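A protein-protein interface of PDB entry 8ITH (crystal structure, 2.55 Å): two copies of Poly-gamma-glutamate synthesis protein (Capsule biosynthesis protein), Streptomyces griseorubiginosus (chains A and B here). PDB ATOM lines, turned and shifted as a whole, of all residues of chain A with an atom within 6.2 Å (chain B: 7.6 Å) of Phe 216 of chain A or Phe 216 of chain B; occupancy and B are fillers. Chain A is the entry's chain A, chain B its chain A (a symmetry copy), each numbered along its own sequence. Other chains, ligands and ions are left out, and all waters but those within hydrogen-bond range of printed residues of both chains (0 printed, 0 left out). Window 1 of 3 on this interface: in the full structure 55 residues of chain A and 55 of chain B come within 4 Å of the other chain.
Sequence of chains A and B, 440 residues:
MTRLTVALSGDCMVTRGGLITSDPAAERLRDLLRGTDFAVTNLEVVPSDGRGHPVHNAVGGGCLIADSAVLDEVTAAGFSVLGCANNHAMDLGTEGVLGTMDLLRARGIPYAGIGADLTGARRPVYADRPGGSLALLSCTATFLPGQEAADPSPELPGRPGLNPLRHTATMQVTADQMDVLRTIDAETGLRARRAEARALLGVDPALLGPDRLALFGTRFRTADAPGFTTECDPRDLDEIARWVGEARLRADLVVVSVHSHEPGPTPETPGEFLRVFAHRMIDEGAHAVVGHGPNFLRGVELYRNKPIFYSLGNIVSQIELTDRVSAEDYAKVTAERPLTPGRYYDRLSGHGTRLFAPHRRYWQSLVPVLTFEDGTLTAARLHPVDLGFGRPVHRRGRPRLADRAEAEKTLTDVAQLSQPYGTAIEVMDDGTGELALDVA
Of the 18 printed residues of chain B, 8 touch a printed residue of chain A.
Hydrophobic or aromatic side chains of chain B within 4 Å of the printed part of chain A: Met 171, Val 173, Leu 181, Ile 184, Leu 190 and Phe 216.
Hydrophobic or aromatic side chains of chain A within 4 Å of the printed part of chain B: Met 171, Leu 181, Ile 184, Leu 190 and Phe 216.
Among the printed residues, no Asp or Glu carboxylate lies within 4 Å of a Lys or Arg side-chain nitrogen of the other chain.
O of Ile 184 of chain B sits at hydrogen-bond distance from OG1 of Thr 188 of chain B (2.6 Å).
The backbone carbonyl oxygen (O) of Asp 185 of chain B is in hydrogen-bond range of the backbone NH (N) of Leu 190 of chain B (3.3 Å).
The backbone carbonyl oxygen of Asp 185 of chain B sits at hydrogen-bond distance from the side-chain hydroxyl of Thr 188 of chain B, at 3.5 Å.
O of Phe 216 of chain A is in hydrogen-bond range of OG1 of Thr 218 of chain A, at 3.2 Å.
O of Phe 216 of chain B is in hydrogen-bond range of OG1 of Thr 218 of chain B, at 3.2 Å.
The backbone carbonyl oxygen of Asp 185 of chain A is in hydrogen-bond range of the backbone NH of Leu 190 of chain A (3.3 Å).
O of Phe 216 of chain B lies close to O of Phe 216 of chain A.
Thr 188 of chain B touches Met 171 of chain A.
CE of Met 171 of chain A touches CD2 of Leu 190 of chain B (3.7 Å).
Leu 181 of chain A touches Leu 181 of chain B (CD2 to CD2, 3.8 Å).
CD2 of Leu 181 of chain A touches CD1 of Ile 184 of chain B, at 3.9 Å.
CG1 of Val 173 of chain B touches CG2 of Ile 184 of chain A, 3.7 Å away.
Ile 184 of chain A touches Leu 181 of chain B (CD1 to CD2, 3.9 Å).
Met 171 of chain B touches Leu 190 of chain A.
Met 171 of chain B touches Phe 216 of chain A (CE to CE1, 3.5 Å).
Phe 216 of chain A touches Thr 218 of chain B (CB to OG1, 3.2 Å).
Thr 218 of chain A touches Phe 216 of chain B (OG1 to CB, 3.2 Å).
Printed residues of chain B within 4 Å of Leu 190 of chain A: Met 171.
Printed residues of chain A within 4 Å of Leu 181 of chain B: Leu 181 and Ile 184.
Printed residues of chain A within 4 Å of Ile 184 of chain B: Leu 181.
Of the printed residues of chain A, Leu 190 of chain B touches Met 171 (3.7 Å).
Printed residues of chain A within 4 Å of Phe 216 of chain B: Met 171 (3.5 Å), Phe 216 (2.7 Å) and Thr 218 (3.2 Å).
The nearest printed residue of chain B that does not touch Phe 216 of chain A is Phe 220 of chain B (4.02 Å).
The nearest printed residue of chain A that does not touch Met 171 of chain B is Ile 184 of chain A (4.5 Å).
Met 171 of chain A touches Leu 190 of chain B, and with the chains exchanged Leu 190 of chain A touches Met 171 of chain B.
Met 171 of chain A touches Phe 216 of chain B, and with the chains exchanged Phe 216 of chain A touches Met 171 of chain B.
Phe 216 of chain B touches its own counterpart, Phe 216 of chain A.
Phe 216 of chain A touches Thr 218 of chain B, and with the chains exchanged Thr 218 of chain A touches Phe 216 of chain B.
Positions printed for both chains: 171, 181, 184, 185, 190, 214, 215, 216, 217, 218 and 220.
Of the 12 pairs that touch across the chains among the printed residues, 10 have their exchanged pair printed and touching as well.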
ATOM      1  N   MET A 171     -28.845 -11.240 -15.666  1.00  0.00           N
ATOM      2  CA  MET A 171     -29.928 -12.084 -16.150  1.00  0.00           C
ATOM      3  C   MET A 171     -30.093 -13.270 -15.208  1.00  0.00           C
ATOM      4  O   MET A 171     -29.185 -14.097 -15.076  1.00  0.00           O
ATOM      5  CB  MET A 171     -29.638 -12.560 -17.572  1.00  0.00           C
ATOM      6  CG  MET A 171     -29.381 -11.436 -18.560  1.00  0.00           C
ATOM      7  SD  MET A 171     -30.896 -10.792 -19.287  1.00  0.00           S
ATOM      8  CE  MET A 171     -31.242 -12.045 -20.519  1.00  0.00           C
ATOM      9  N   LEU A 181     -26.585 -22.795 -21.377  1.00  0.00           N
ATOM     10  CA  LEU A 181     -25.680 -21.712 -21.747  1.00  0.00           C
ATOM     11  C   LEU A 181     -24.229 -22.177 -21.731  1.00  0.00           C
ATOM     12  O   LEU A 181     -23.468 -21.909 -22.668  1.00  0.00           O
ATOM     13  CB  LEU A 181     -25.877 -20.520 -20.810  1.00  0.00           C
ATOM     14  CG  LEU A 181     -27.210 -19.783 -20.936  1.00  0.00           C
ATOM     15  CD1 LEU A 181     -27.325 -18.704 -19.874  1.00  0.00           C
ATOM     16  CD2 LEU A 181     -27.361 -19.187 -22.327  1.00  0.00           C
ATOM     17  N   ILE A 184     -23.685 -24.510 -24.643  1.00  0.00           N
ATOM     18  CA  ILE A 184     -23.459 -23.720 -25.851  1.00  0.00           C
ATOM     19  C   ILE A 184     -22.052 -23.138 -25.845  1.00  0.00           C
ATOM     20  O   ILE A 184     -21.383 -23.078 -26.882  1.00  0.00           O
ATOM     21  CB  ILE A 184     -24.529 -22.619 -25.977  1.00  0.00           C
ATOM     22  CG1 ILE A 184     -25.910 -23.234 -26.213  1.00  0.00           C
ATOM     23  CG2 ILE A 184     -24.181 -21.647 -27.096  1.00  0.00           C
ATOM     24  CD1 ILE A 184     -27.030 -22.218 -26.229  1.00  0.00           C
ATOM     25  N   ASP A 185     -21.574 -22.718 -24.671  1.00  0.00           N
ATOM     26  CA  ASP A 185     -20.228 -22.164 -24.567  1.00  0.00           C
ATOM     27  C   ASP A 185     -19.174 -23.191 -24.960  1.00  0.00           C
ATOM     28  O   ASP A 185     -18.244 -22.887 -25.715  1.00  0.00           O
ATOM     29  CB  ASP A 185     -19.983 -21.664 -23.144  1.00  0.00           C
ATOM     30  CG  ASP A 185     -18.556 -21.205 -22.921  1.00  0.00           C
ATOM     31  OD1 ASP A 185     -18.131 -20.230 -23.578  1.00  0.00           O
ATOM     32  OD2 ASP A 185     -17.861 -21.814 -22.081  1.00  0.00           O
ATOM     33  N   LEU A 190     -16.337 -21.728 -28.128  1.00  0.00           N
ATOM     34  CA  LEU A 190     -16.027 -20.432 -27.536  1.00  0.00           C
ATOM     35  C   LEU A 190     -15.152 -20.587 -26.300  1.00  0.00           C
ATOM     36  O   LEU A 190     -14.224 -19.797 -26.087  1.00  0.00           O
ATOM     37  CB  LEU A 190     -17.318 -19.692 -27.186  1.00  0.00           C
ATOM     38  CG  LEU A 190     -17.148 -18.252 -26.699  1.00  0.00           C
ATOM     39  CD1 LEU A 190     -16.816 -17.331 -27.865  1.00  0.00           C
ATOM     40  CD2 LEU A 190     -18.389 -17.775 -25.958  1.00  0.00           C
ATOM     41  N   ALA A 214     -20.347 -15.252 -16.632  1.00  0.00           N
ATOM     42  CA  ALA A 214     -20.220 -14.134 -17.567  1.00  0.00           C
ATOM     43  C   ALA A 214     -19.919 -14.683 -18.955  1.00  0.00           C
ATOM     44  O   ALA A 214     -18.815 -15.177 -19.203  1.00  0.00           O
ATOM     45  CB  ALA A 214     -19.130 -13.158 -17.127  1.00  0.00           C
ATOM     46  N   LEU A 215     -20.897 -14.590 -19.855  1.00  0.00           N
ATOM     47  CA  LEU A 215     -20.738 -15.036 -21.231  1.00  0.00           C
ATOM     48  C   LEU A 215     -21.393 -14.028 -22.160  1.00  0.00           C
ATOM     49  O   LEU A 215     -22.362 -13.360 -21.792  1.00  0.00           O
ATOM     50  CB  LEU A 215     -21.356 -16.417 -21.481  1.00  0.00           C
ATOM     51  CG  LEU A 215     -20.796 -17.628 -20.740  1.00  0.00           C
ATOM     52  CD1 LEU A 215     -21.326 -17.664 -19.338  1.00  0.00           C
ATOM     53  CD2 LEU A 215     -21.175 -18.894 -21.464  1.00  0.00           C
ATOM     54  N   PHE A 216     -20.858 -13.938 -23.378  1.00  0.00           N
ATOM     55  CA  PHE A 216     -21.356 -13.011 -24.392  1.00  0.00           C
ATOM     56  C   PHE A 216     -21.397 -11.580 -23.864  1.00  0.00           C
ATOM     57  O   PHE A 216     -22.265 -10.790 -24.240  1.00  0.00           O
ATOM     58  CB  PHE A 216     -22.738 -13.430 -24.905  1.00  0.00           C
ATOM     59  CG  PHE A 216     -22.952 -14.916 -24.935  1.00  0.00           C
ATOM     60  CD1 PHE A 216     -22.139 -15.735 -25.702  1.00  0.00           C
ATOM     61  CD2 PHE A 216     -23.981 -15.493 -24.210  1.00  0.00           C
ATOM     62  CE1 PHE A 216     -22.339 -17.103 -25.733  1.00  0.00           C
ATOM     63  CE2 PHE A 216     -24.189 -16.860 -24.238  1.00  0.00           C
ATOM     64  CZ  PHE A 216     -23.366 -17.666 -25.001  1.00  0.00           C
ATOM     65  N   GLY A 217     -20.459 -11.240 -22.982  1.00  0.00           N
ATOM     66  CA  GLY A 217     -20.471  -9.933 -22.351  1.00  0.00           C
ATOM     67  C   GLY A 217     -21.711  -9.667 -21.530  1.00  0.00           C
ATOM     68  O   GLY A 217     -22.168  -8.521 -21.458  1.00  0.00           O
ATOM     69  N   THR A 218     -22.279 -10.703 -20.918  1.00  0.00           N
ATOM     70  CA  THR A 218     -23.495 -10.580 -20.128  1.00  0.00           C
ATOM     71  C   THR A 218     -23.350 -11.419 -18.868  1.00  0.00           C
ATOM     72  O   THR A 218     -22.747 -12.495 -18.896  1.00  0.00           O
ATOM     73  CB  THR A 218     -24.729 -11.028 -20.924  1.00  0.00           C
ATOM     74  OG1 THR A 218     -24.742 -10.364 -22.193  1.00  0.00           O
ATOM     75  CG2 THR A 218     -26.010 -10.687 -20.173  1.00  0.00           C
ATOM     76  N   PHE A 220     -24.843 -13.754 -15.996  1.00  0.00           N
ATOM     77  CA  PHE A 220     -25.923 -14.693 -15.728  1.00  0.00           C
ATOM     78  C   PHE A 220     -25.806 -15.222 -14.305  1.00  0.00           C
ATOM     79  O   PHE A 220     -24.703 -15.393 -13.777  1.00  0.00           O
ATOM     80  CB  PHE A 220     -25.910 -15.864 -16.724  1.00  0.00           C
ATOM     81  CG  PHE A 220     -26.252 -15.468 -18.133  1.00  0.00           C
ATOM     82  CD1 PHE A 220     -27.570 -15.312 -18.527  1.00  0.00           C
ATOM     83  CD2 PHE A 220     -25.252 -15.263 -19.069  1.00  0.00           C
ATOM     84  CE1 PHE A 220     -27.886 -14.950 -19.825  1.00  0.00           C
ATOM     85  CE2 PHE A 220     -25.558 -14.903 -20.366  1.00  0.00           C
ATOM     86  CZ  PHE A 220     -26.877 -14.745 -20.746  1.00  0.00           C
ATOM     87  N   MET B 171     -22.027 -17.343 -33.608  1.00  0.00           N
ATOM     88  CA  MET B 171     -22.124 -18.589 -32.862  1.00  0.00           C
ATOM     89  C   MET B 171     -23.142 -19.497 -33.542  1.00  0.00           C
ATOM     90  O   MET B 171     -24.331 -19.165 -33.612  1.00  0.00           O
ATOM     91  CB  MET B 171     -22.528 -18.313 -31.414  1.00  0.00           C
ATOM     92  CG  MET B 171     -21.605 -17.350 -30.689  1.00  0.00           C
ATOM     93  SD  MET B 171     -20.193 -18.175 -29.939  1.00  0.00           S
ATOM     94  CE  MET B 171     -20.942 -18.860 -28.464  1.00  0.00           C
ATOM     95  N   VAL B 173     -25.436 -22.589 -33.442  1.00  0.00           N
ATOM     96  CA  VAL B 173     -26.089 -23.395 -32.418  1.00  0.00           C
ATOM     97  C   VAL B 173     -27.160 -24.256 -33.068  1.00  0.00           C
ATOM     98  O   VAL B 173     -27.702 -23.920 -34.127  1.00  0.00           O
ATOM     99  CB  VAL B 173     -26.701 -22.529 -31.291  1.00  0.00           C
ATOM    100  CG1 VAL B 173     -25.610 -21.804 -30.520  1.00  0.00           C
ATOM    101  CG2 VAL B 173     -27.707 -21.541 -31.862  1.00  0.00           C
ATOM    102  N   VAL B 180     -33.908 -22.358 -26.694  1.00  0.00           N
ATOM    103  CA  VAL B 180     -33.640 -22.046 -25.293  1.00  0.00           C
ATOM    104  C   VAL B 180     -33.182 -20.600 -25.149  1.00  0.00           C
ATOM    105  O   VAL B 180     -33.556 -19.908 -24.194  1.00  0.00           O
ATOM    106  CB  VAL B 180     -32.609 -23.030 -24.711  1.00  0.00           C
ATOM    107  CG1 VAL B 180     -32.258 -22.653 -23.277  1.00  0.00           C
ATOM    108  CG2 VAL B 180     -33.141 -24.450 -24.772  1.00  0.00           C
ATOM    109  N   LEU B 181     -32.380 -20.115 -26.100  1.00  0.00           N
ATOM    110  CA  LEU B 181     -31.896 -18.739 -26.038  1.00  0.00           C
ATOM    111  C   LEU B 181     -33.049 -17.746 -26.121  1.00  0.00           C
ATOM    112  O   LEU B 181     -33.120 -16.792 -25.336  1.00  0.00           O
ATOM    113  CB  LEU B 181     -30.884 -18.488 -27.156  1.00  0.00           C
ATOM    114  CG  LEU B 181     -29.551 -19.226 -27.030  1.00  0.00           C
ATOM    115  CD1 LEU B 181     -28.691 -18.985 -28.257  1.00  0.00           C
ATOM    116  CD2 LEU B 181     -28.821 -18.794 -25.768  1.00  0.00           C
ATOM    117  N   ARG B 182     -33.969 -17.955 -27.066  1.00  0.00           N
ATOM    118  CA  ARG B 182     -35.119 -17.064 -27.164  1.00  0.00           C
ATOM    119  C   ARG B 182     -36.059 -17.226 -25.979  1.00  0.00           C
ATOM    120  O   ARG B 182     -36.708 -16.257 -25.570  1.00  0.00           O
ATOM    121  CB  ARG B 182     -35.866 -17.303 -28.474  1.00  0.00           C
ATOM    122  CG  ARG B 182     -35.100 -16.803 -29.669  1.00  0.00           C
ATOM    123  CD  ARG B 182     -35.952 -16.674 -30.918  1.00  0.00           C
ATOM    124  NE  ARG B 182     -36.438 -17.965 -31.384  1.00  0.00           N
ATOM    125  CZ  ARG B 182     -36.622 -18.270 -32.664  1.00  0.00           C
ATOM    126  NH1 ARG B 182     -37.074 -19.470 -33.002  1.00  0.00           N
ATOM    127  NH2 ARG B 182     -36.341 -17.379 -33.605  1.00  0.00           N
ATOM    128  N   ILE B 184     -34.998 -17.900 -22.897  1.00  0.00           N
ATOM    129  CA  ILE B 184     -34.319 -17.088 -21.889  1.00  0.00           C
ATOM    130  C   ILE B 184     -34.562 -15.609 -22.154  1.00  0.00           C
ATOM    131  O   ILE B 184     -34.750 -14.817 -21.224  1.00  0.00           O
ATOM    132  CB  ILE B 184     -32.815 -17.422 -21.860  1.00  0.00           C
ATOM    133  CG1 ILE B 184     -32.589 -18.853 -21.367  1.00  0.00           C
ATOM    134  CG2 ILE B 184     -32.056 -16.432 -20.987  1.00  0.00           C
ATOM    135  CD1 ILE B 184     -31.144 -19.291 -21.423  1.00  0.00           C
ATOM    136  N   ASP B 185     -34.580 -15.216 -23.430  1.00  0.00           N
ATOM    137  CA  ASP B 185     -34.825 -13.819 -23.779  1.00  0.00           C
ATOM    138  C   ASP B 185     -36.202 -13.365 -23.314  1.00  0.00           C
ATOM    139  O   ASP B 185     -36.350 -12.285 -22.733  1.00  0.00           O
ATOM    140  CB  ASP B 185     -34.681 -13.631 -25.288  1.00  0.00           C
ATOM    141  CG  ASP B 185     -35.060 -12.236 -25.743  1.00  0.00           C
ATOM    142  OD1 ASP B 185     -34.387 -11.267 -25.330  1.00  0.00           O
ATOM    143  OD2 ASP B 185     -36.028 -12.109 -26.523  1.00  0.00           O
ATOM    144  N   THR B 188     -36.846 -13.957 -19.049  1.00  0.00           N
ATOM    145  CA  THR B 188     -36.144 -13.044 -18.153  1.00  0.00           C
ATOM    146  C   THR B 188     -36.692 -11.625 -18.212  1.00  0.00           C
ATOM    147  O   THR B 188     -36.325 -10.803 -17.366  1.00  0.00           O
ATOM    148  CB  THR B 188     -34.645 -13.016 -18.467  1.00  0.00           C
ATOM    149  OG1 THR B 188     -34.447 -12.649 -19.838  1.00  0.00           O
ATOM    150  CG2 THR B 188     -34.009 -14.376 -18.201  1.00  0.00           C
ATOM    151  N   LEU B 190     -36.108  -9.639 -20.797  1.00  0.00           N
ATOM    152  CA  LEU B 190     -35.236  -8.842 -21.652  1.00  0.00           C
ATOM    153  C   LEU B 190     -35.954  -8.412 -22.922  1.00  0.00           C
ATOM    154  O   LEU B 190     -35.793  -7.273 -23.377  1.00  0.00           O
ATOM    155  CB  LEU B 190     -33.973  -9.632 -21.995  1.00  0.00           C
ATOM    156  CG  LEU B 190     -32.895  -8.863 -22.759  1.00  0.00           C
ATOM    157  CD1 LEU B 190     -32.165  -7.903 -21.829  1.00  0.00           C
ATOM    158  CD2 LEU B 190     -31.922  -9.815 -23.441  1.00  0.00           C
ATOM    159  N   ARG B 194     -37.034  -4.271 -24.897  1.00  0.00           N
ATOM    160  CA  ARG B 194     -36.849  -3.785 -26.257  1.00  0.00           C
ATOM    161  C   ARG B 194     -38.158  -3.311 -26.881  1.00  0.00           C
ATOM    162  O   ARG B 194     -38.216  -3.107 -28.099  1.00  0.00           O
ATOM    163  CB  ARG B 194     -36.222  -4.874 -27.135  1.00  0.00           C
ATOM    164  CG  ARG B 194     -34.867  -5.365 -26.662  1.00  0.00           C
ATOM    165  CD  ARG B 194     -34.171  -6.189 -27.739  1.00  0.00           C
ATOM    166  NE  ARG B 194     -34.997  -7.296 -28.213  1.00  0.00           N
ATOM    167  CZ  ARG B 194     -34.989  -8.514 -27.684  1.00  0.00           C
ATOM    168  NH1 ARG B 194     -34.195  -8.787 -26.657  1.00  0.00           N
ATOM    169  NH2 ARG B 194     -35.777  -9.460 -28.179  1.00  0.00           N
ATOM    170  N   ALA B 206     -33.487  -7.683 -32.575  1.00  0.00           N
ATOM    171  CA  ALA B 206     -32.930  -8.990 -32.261  1.00  0.00           C
ATOM    172  C   ALA B 206     -33.364 -10.071 -33.242  1.00  0.00           C
ATOM    173  O   ALA B 206     -32.811 -11.175 -33.208  1.00  0.00           O
ATOM    174  CB  ALA B 206     -33.324  -9.404 -30.840  1.00  0.00           C
ATOM    175  N   ALA B 214     -29.755 -11.967 -32.813  1.00  0.00           N
ATOM    176  CA  ALA B 214     -28.776 -11.127 -32.124  1.00  0.00           C
ATOM    177  C   ALA B 214     -29.250 -10.885 -30.698  1.00  0.00           C
ATOM    178  O   ALA B 214     -30.218 -10.151 -30.479  1.00  0.00           O
ATOM    179  CB  ALA B 214     -28.565  -9.801 -32.853  1.00  0.00           C
ATOM    180  N   LEU B 215     -28.566 -11.498 -29.732  1.00  0.00           N
ATOM    181  CA  LEU B 215     -28.880 -11.326 -28.322  1.00  0.00           C
ATOM    182  C   LEU B 215     -27.587 -11.204 -27.535  1.00  0.00           C
ATOM    183  O   LEU B 215     -26.554 -11.761 -27.917  1.00  0.00           O
ATOM    184  CB  LEU B 215     -29.700 -12.491 -27.752  1.00  0.00           C
ATOM    185  CG  LEU B 215     -31.096 -12.759 -28.307  1.00  0.00           C
ATOM    186  CD1 LEU B 215     -30.999 -13.490 -29.613  1.00  0.00           C
ATOM    187  CD2 LEU B 215     -31.892 -13.575 -27.322  1.00  0.00           C
ATOM    188  N   PHE B 216     -27.661 -10.477 -26.419  1.00  0.00           N
ATOM    189  CA  PHE B 216     -26.508 -10.246 -25.550  1.00  0.00           C
ATOM    190  C   PHE B 216     -25.332  -9.667 -26.331  1.00  0.00           C
ATOM    191  O   PHE B 216     -24.170  -9.938 -26.020  1.00  0.00           O
ATOM    192  CB  PHE B 216     -26.086 -11.528 -24.824  1.00  0.00           C
ATOM    193  CG  PHE B 216     -27.230 -12.444 -24.492  1.00  0.00           C
ATOM    194  CD1 PHE B 216     -28.265 -12.020 -23.676  1.00  0.00           C
ATOM    195  CD2 PHE B 216     -27.258 -13.738 -24.983  1.00  0.00           C
ATOM    196  CE1 PHE B 216     -29.316 -12.865 -23.368  1.00  0.00           C
ATOM    197  CE2 PHE B 216     -28.303 -14.591 -24.676  1.00  0.00           C
ATOM    198  CZ  PHE B 216     -29.334 -14.153 -23.868  1.00  0.00           C
ATOM    199  N   GLY B 217     -25.627  -8.870 -27.355  1.00  0.00           N
ATOM    200  CA  GLY B 217     -24.581  -8.347 -28.216  1.00  0.00           C
ATOM    201  C   GLY B 217     -23.796  -9.418 -28.936  1.00  0.00           C
ATOM    202  O   GLY B 217     -22.596  -9.248 -29.174  1.00  0.00           O
ATOM    203  N   THR B 218     -24.442 -10.531 -29.279  1.00  0.00           N
ATOM    204  CA  THR B 218     -23.787 -11.647 -29.944  1.00  0.00           C
ATOM    205  C   THR B 218     -24.706 -12.179 -31.032  1.00  0.00           C
ATOM    206  O   THR B 218     -25.929 -12.200 -30.866  1.00  0.00           O
ATOM    207  CB  THR B 218     -23.437 -12.765 -28.951  1.00  0.00           C
ATOM    208  OG1 THR B 218     -22.734 -12.207 -27.836  1.00  0.00           O
ATOM    209  CG2 THR B 218     -22.560 -13.821 -29.613  1.00  0.00           C
ATOM    210  N   ARG B 219     -24.115 -12.604 -32.145  1.00  0.00           N
ATOM    211  CA  ARG B 219     -24.877 -13.117 -33.272  1.00  0.00           C
ATOM    212  C   ARG B 219     -24.980 -14.635 -33.180  1.00  0.00           C
ATOM    213  O   ARG B 219     -23.963 -15.325 -33.054  1.00  0.00           O
ATOM    214  CB  ARG B 219     -24.227 -12.702 -34.591  1.00  0.00           C
ATOM    215  CG  ARG B 219     -24.044 -11.200 -34.735  1.00  0.00           C
ATOM    216  CD  ARG B 219     -23.014 -10.858 -35.803  1.00  0.00           C
ATOM    217  NE  ARG B 219     -23.614 -10.254 -36.990  1.00  0.00           N
ATOM    218  CZ  ARG B 219     -23.822  -8.949 -37.141  1.00  0.00           C
ATOM    219  NH1 ARG B 219     -23.483  -8.106 -36.176  1.00  0.00           N
ATOM    220  NH2 ARG B 219     -24.369  -8.485 -38.257  1.00  0.00           N
ATOM    221  N   PHE B 220     -26.208 -15.147 -33.238  1.00  0.00           N
ATOM    222  CA  PHE B 220     -26.468 -16.579 -33.208  1.00  0.00           C
ATOM    223  C   PHE B 220     -27.128 -17.011 -34.511  1.00  0.00           C
ATOM    224  O   PHE B 220     -27.904 -16.262 -35.111  1.00  0.00           O
ATOM    225  CB  PHE B 220     -27.360 -16.964 -32.018  1.00  0.00           C
ATOM    226  CG  PHE B 220     -26.697 -16.790 -30.680  1.00  0.00           C
ATOM    227  CD1 PHE B 220     -25.835 -17.755 -30.185  1.00  0.00           C
ATOM    228  CD2 PHE B 220     -26.946 -15.666 -29.911  1.00  0.00           C
ATOM    229  CE1 PHE B 220     -25.226 -17.597 -28.952  1.00  0.00           C
ATOM    230  CE2 PHE B 220     -26.344 -15.502 -28.680  1.00  0.00           C
ATOM    231  CZ  PHE B 220     -25.481 -16.469 -28.198  1.00  0.00           C
